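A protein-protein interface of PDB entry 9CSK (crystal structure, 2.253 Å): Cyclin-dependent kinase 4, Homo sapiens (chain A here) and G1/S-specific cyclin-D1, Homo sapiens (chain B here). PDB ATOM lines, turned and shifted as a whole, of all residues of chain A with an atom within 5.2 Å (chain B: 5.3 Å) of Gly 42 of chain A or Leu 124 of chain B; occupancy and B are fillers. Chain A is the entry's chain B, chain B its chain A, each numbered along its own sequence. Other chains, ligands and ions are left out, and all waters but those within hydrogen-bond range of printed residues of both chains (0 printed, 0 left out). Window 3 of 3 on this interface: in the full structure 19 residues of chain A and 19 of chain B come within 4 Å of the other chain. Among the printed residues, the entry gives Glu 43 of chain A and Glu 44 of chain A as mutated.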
ATOM      1  N   PRO A  40     -20.515  -1.120 -15.544  1.00  0.00           N
ATOM      2  CA  PRO A  40     -20.622  -0.748 -14.137  1.00  0.00           C
ATOM      3  C   PRO A  40     -19.322  -0.993 -13.360  1.00  0.00           C
ATOM      4  O   PRO A  40     -18.608  -1.921 -13.677  1.00  0.00           O
ATOM      5  CB  PRO A  40     -21.727  -1.674 -13.615  1.00  0.00           C
ATOM      6  CG  PRO A  40     -21.638  -2.881 -14.515  1.00  0.00           C
ATOM      7  CD  PRO A  40     -21.299  -2.309 -15.873  1.00  0.00           C
ATOM      8  N   ASN A  41     -19.055  -0.132 -12.378  1.00  0.00           N
ATOM      9  CA  ASN A  41     -17.871  -0.244 -11.487  1.00  0.00           C
ATOM     10  C   ASN A  41     -18.360  -0.817 -10.155  1.00  0.00           C
ATOM     11  O   ASN A  41     -18.866  -0.043  -9.331  1.00  0.00           O
ATOM     12  CB  ASN A  41     -17.173   1.104 -11.297  1.00  0.00           C
ATOM     13  CG  ASN A  41     -15.849   0.990 -10.572  1.00  0.00           C
ATOM     14  OD1 ASN A  41     -15.311  -0.101 -10.419  1.00  0.00           O
ATOM     15  ND2 ASN A  41     -15.314   2.115 -10.132  1.00  0.00           N
ATOM     16  N   GLY A  42     -18.271  -2.137  -9.996  1.00  0.00           N
ATOM     17  CA  GLY A  42     -18.748  -2.830  -8.786  1.00  0.00           C
ATOM     18  C   GLY A  42     -17.699  -2.941  -7.696  1.00  0.00           C
ATOM     19  O   GLY A  42     -16.609  -2.369  -7.850  1.00  0.00           O
ATOM     20  N   GLU A  43     -18.046  -3.660  -6.621  1.00  0.00           N
ATOM     21  CA  GLU A  43     -17.148  -3.940  -5.468  1.00  0.00           C
ATOM     22  C   GLU A  43     -15.955  -4.772  -5.952  1.00  0.00           C
ATOM     23  O   GLU A  43     -14.870  -4.639  -5.366  1.00  0.00           O
ATOM     24  CB  GLU A  43     -17.913  -4.635  -4.342  1.00  0.00           C
ATOM     25  CG  GLU A  43     -18.694  -5.846  -4.811  1.00  0.00           C
ATOM     26  CD  GLU A  43     -19.275  -6.691  -3.693  1.00  0.00           C
ATOM     27  OE1 GLU A  43     -19.724  -6.110  -2.691  1.00  0.00           O
ATOM     28  OE2 GLU A  43     -19.269  -7.927  -3.827  1.00  0.00           O
ATOM     29  N   GLU A  44     -16.169  -5.592  -6.985  1.00  0.00           N
ATOM     30  CA  GLU A  44     -15.110  -6.478  -7.537  1.00  0.00           C
ATOM     31  C   GLU A  44     -14.428  -5.810  -8.734  1.00  0.00           C
ATOM     32  O   GLU A  44     -13.804  -6.537  -9.519  1.00  0.00           O
ATOM     33  CB  GLU A  44     -15.701  -7.840  -7.900  1.00  0.00           C
ATOM     34  CG  GLU A  44     -16.120  -8.645  -6.684  1.00  0.00           C
ATOM     35  CD  GLU A  44     -15.033  -8.814  -5.636  1.00  0.00           C
ATOM     36  OE1 GLU A  44     -15.364  -8.844  -4.439  1.00  0.00           O
ATOM     37  OE2 GLU A  44     -13.862  -8.918  -6.023  1.00  0.00           O
ATOM     38  N   GLY A  45     -14.481  -4.475  -8.793  1.00  0.00           N
ATOM     39  CA  GLY A  45     -13.859  -3.652  -9.851  1.00  0.00           C
ATOM     40  C   GLY A  45     -14.432  -3.901 -11.234  1.00  0.00           C
ATOM     41  O   GLY A  45     -15.662  -3.841 -11.380  1.00  0.00           O
ATOM     42  N   PHE B  94      -5.859 -11.693  -9.168  1.00  0.00           N
ATOM     43  CA  PHE B  94      -7.228 -11.242  -9.277  1.00  0.00           C
ATOM     44  C   PHE B  94      -7.696 -11.271 -10.737  1.00  0.00           C
ATOM     45  O   PHE B  94      -8.758 -11.813 -11.012  1.00  0.00           O
ATOM     46  CB  PHE B  94      -7.296  -9.815  -8.706  1.00  0.00           C
ATOM     47  CG  PHE B  94      -8.657  -9.179  -8.596  1.00  0.00           C
ATOM     48  CD1 PHE B  94      -9.669  -9.796  -7.882  1.00  0.00           C
ATOM     49  CD2 PHE B  94      -8.895  -7.923  -9.127  1.00  0.00           C
ATOM     50  CE1 PHE B  94     -10.902  -9.186  -7.730  1.00  0.00           C
ATOM     51  CE2 PHE B  94     -10.130  -7.311  -8.975  1.00  0.00           C
ATOM     52  CZ  PHE B  94     -11.126  -7.942  -8.271  1.00  0.00           C
ATOM     53  N   ALA B 107     -11.554  -9.590  -4.138  1.00  0.00           N
ATOM     54  CA  ALA B 107     -10.516  -8.661  -3.745  1.00  0.00           C
ATOM     55  C   ALA B 107     -10.196  -8.792  -2.257  1.00  0.00           C
ATOM     56  O   ALA B 107      -9.033  -8.783  -1.866  1.00  0.00           O
ATOM     57  CB  ALA B 107     -10.957  -7.248  -4.073  1.00  0.00           C
ATOM     58  N   PRO B 120      -9.250  -3.668  -0.592  1.00  0.00           N
ATOM     59  CA  PRO B 120      -9.852  -3.896  -1.922  1.00  0.00           C
ATOM     60  C   PRO B 120      -9.790  -2.724  -2.889  1.00  0.00           C
ATOM     61  O   PRO B 120      -9.467  -2.938  -4.045  1.00  0.00           O
ATOM     62  CB  PRO B 120     -11.296  -4.286  -1.610  1.00  0.00           C
ATOM     63  CG  PRO B 120     -11.237  -4.863  -0.253  1.00  0.00           C
ATOM     64  CD  PRO B 120     -10.156  -4.115   0.486  1.00  0.00           C
ATOM     65  N   GLU B 121     -10.016  -1.496  -2.420  1.00  0.00           N
ATOM     66  CA  GLU B 121      -9.965  -0.281  -3.228  1.00  0.00           C
ATOM     67  C   GLU B 121      -8.638  -0.160  -3.980  1.00  0.00           C
ATOM     68  O   GLU B 121      -8.647   0.096  -5.179  1.00  0.00           O
ATOM     69  CB  GLU B 121     -10.192   0.956  -2.339  1.00  0.00           C
ATOM     70  CG  GLU B 121     -11.565   1.012  -1.679  1.00  0.00           C
ATOM     71  CD  GLU B 121     -11.808   0.120  -0.468  1.00  0.00           C
ATOM     72  OE1 GLU B 121     -10.816  -0.320   0.162  1.00  0.00           O
ATOM     73  OE2 GLU B 121     -12.994  -0.144  -0.153  1.00  0.00           O
ATOM     74  N   GLU B 122      -7.510  -0.414  -3.289  1.00  0.00           N
ATOM     75  CA  GLU B 122      -6.168  -0.362  -3.878  1.00  0.00           C
ATOM     76  C   GLU B 122      -5.975  -1.423  -4.958  1.00  0.00           C
ATOM     77  O   GLU B 122      -5.270  -1.203  -5.956  1.00  0.00           O
ATOM     78  CB  GLU B 122      -5.113  -0.558  -2.793  1.00  0.00           C
ATOM     79  CG  GLU B 122      -5.132   0.494  -1.706  1.00  0.00           C
ATOM     80  CD  GLU B 122      -4.042   0.221  -0.689  1.00  0.00           C
ATOM     81  OE1 GLU B 122      -3.987  -0.916  -0.174  1.00  0.00           O
ATOM     82  OE2 GLU B 122      -3.212   1.123  -0.440  1.00  0.00           O
ATOM     83  N   LEU B 123      -6.558  -2.595  -4.730  1.00  0.00           N
ATOM     84  CA  LEU B 123      -6.493  -3.684  -5.674  1.00  0.00           C
ATOM     85  C   LEU B 123      -7.337  -3.345  -6.926  1.00  0.00           C
ATOM     86  O   LEU B 123      -6.921  -3.667  -8.033  1.00  0.00           O
ATOM     87  CB  LEU B 123      -6.964  -4.975  -4.985  1.00  0.00           C
ATOM     88  CG  LEU B 123      -6.271  -6.265  -5.415  1.00  0.00           C
ATOM     89  CD1 LEU B 123      -6.379  -7.330  -4.361  1.00  0.00           C
ATOM     90  CD2 LEU B 123      -6.891  -6.785  -6.607  1.00  0.00           C
ATOM     91  N   LEU B 124      -8.482  -2.670  -6.766  1.00  0.00           N
ATOM     92  CA  LEU B 124      -9.311  -2.303  -7.908  1.00  0.00           C
ATOM     93  C   LEU B 124      -8.663  -1.208  -8.764  1.00  0.00           C
ATOM     94  O   LEU B 124      -8.809  -1.229  -9.996  1.00  0.00           O
ATOM     95  CB  LEU B 124     -10.734  -1.930  -7.490  1.00  0.00           C
ATOM     96  CG  LEU B 124     -11.490  -2.949  -6.627  1.00  0.00           C
ATOM     97  CD1 LEU B 124     -12.904  -2.471  -6.353  1.00  0.00           C
ATOM     98  CD2 LEU B 124     -11.458  -4.380  -7.226  1.00  0.00           C
ATOM     99  N   GLN B 125      -7.883  -0.305  -8.131  1.00  0.00           N
ATOM    100  CA  GLN B 125      -7.157   0.742  -8.846  1.00  0.00           C
ATOM    101  C   GLN B 125      -6.004   0.122  -9.626  1.00  0.00           C
ATOM    102  O   GLN B 125      -5.763   0.509 -10.764  1.00  0.00           O
ATOM    103  CB  GLN B 125      -6.629   1.818  -7.883  1.00  0.00           C
ATOM    104  CG  GLN B 125      -7.662   2.844  -7.480  1.00  0.00           C
ATOM    105  CD  GLN B 125      -7.166   3.825  -6.414  1.00  0.00           C
ATOM    106  OE1 GLN B 125      -7.937   4.271  -5.542  1.00  0.00           O
ATOM    107  NE2 GLN B 125      -5.880   4.199  -6.464  1.00  0.00           N
ATOM    108  N   MET B 126      -5.339  -0.855  -9.014  1.00  0.00           N
ATOM    109  CA  MET B 126      -4.231  -1.575  -9.686  1.00  0.00           C
ATOM    110  C   MET B 126      -4.799  -2.317 -10.903  1.00  0.00           C
ATOM    111  O   MET B 126      -4.116  -2.346 -11.943  1.00  0.00           O
ATOM    112  CB  MET B 126      -3.580  -2.578  -8.729  1.00  0.00           C
ATOM    113  CG  MET B 126      -2.187  -2.992  -9.155  1.00  0.00           C
ATOM    114  SD  MET B 126      -1.123  -1.570  -9.496  1.00  0.00           S
ATOM    115  CE  MET B 126       0.281  -2.381 -10.257  1.00  0.00           C
ATOM    116  N   GLU B 127      -6.018  -2.858 -10.782  1.00  0.00           N
ATOM    117  CA  GLU B 127      -6.617  -3.652 -11.857  1.00  0.00           C
ATOM    118  C   GLU B 127      -6.710  -2.855 -13.144  1.00  0.00           C
ATOM    119  O   GLU B 127      -6.410  -3.389 -14.210  1.00  0.00           O
ATOM    120  CB  GLU B 127      -7.999  -4.179 -11.457  1.00  0.00           C
ATOM    121  CG  GLU B 127      -8.648  -4.998 -12.549  1.00  0.00           C
ATOM    122  CD  GLU B 127     -10.057  -5.476 -12.262  1.00  0.00           C
ATOM    123  OE1 GLU B 127     -10.887  -4.663 -11.789  1.00  0.00           O
ATOM    124  OE2 GLU B 127     -10.334  -6.668 -12.536  1.00  0.00           O
ATOM    125  N   LEU B 128      -7.113  -1.576 -13.051  1.00  0.00           N
ATOM    126  CA  LEU B 128      -7.190  -0.724 -14.233  1.00  0.00           C
ATOM    127  C   LEU B 128      -5.818  -0.483 -14.816  1.00  0.00           C
ATOM    128  O   LEU B 128      -5.653  -0.587 -16.022  1.00  0.00           O
ATOM    129  CB  LEU B 128      -7.878   0.605 -13.933  1.00  0.00           C
ATOM    130  CG  LEU B 128      -9.360   0.518 -13.613  1.00  0.00           C
ATOM    131  CD1 LEU B 128      -9.929   1.892 -13.434  1.00  0.00           C
ATOM    132  CD2 LEU B 128     -10.128  -0.155 -14.714  1.00  0.00           C
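Among the printed residues, merely in contact across the chains: Gly 42 of chain A with Leu 124 of chain B, Glu 43 of chain A with Leu 124 of chain B, Glu 44 of chain A with Phe 94 of chain B, Glu 44 of chain A with Leu 124 of chain B, Gly 45 of chain A with Leu 124 of chain B and Gly 45 of chain A with Glu 127 of chain B.
Printed residues of chain A that touch a printed residue of chain B: Gly 42, Glu 43, Glu 44 and Gly 45. Of the 11 printed residues of chain B, 4 touch a printed residue of chain A. Hydrophobic or aromatic side chains of chain B within 4 Å of the printed part of chain A: Phe 94, Ala 107 and Leu 124.
The backbone NH of Ala 107 of chain B is in hydrogen-bond range of the side-chain carboxylate of Glu 44 of chain A (3.1 Å).
Printed residues of chain B within 4 Å of Gly 42 of chain A: Leu 124 (3.997 Å). Of the printed residues of chain B, Glu 43 of chain A touches Leu 124. Of the printed residues of chain B, Gly 45 of chain A touches Leu 124 and Glu 127. Printed residues of chain A within 4 Å of Phe 94 of chain B: Glu 44. Printed residues of chain A within 4 Å of Leu 124 of chain B: Gly 42 (3.997 Å), Glu 43 (3.1 Å), Glu 44 (3.6 Å) and Gly 45 (3.4 Å). Of the printed residues of chain A, Glu 127 of chain B touches Gly 45. The nearest printed residue of chain A that does not touch Leu 124 of chain B is Asn 41 of chain A (5.3 Å). The nearest printed residue of chain A that does not touch Ala 107 of chain B is Glu 43 of chain A (4.9 Å).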
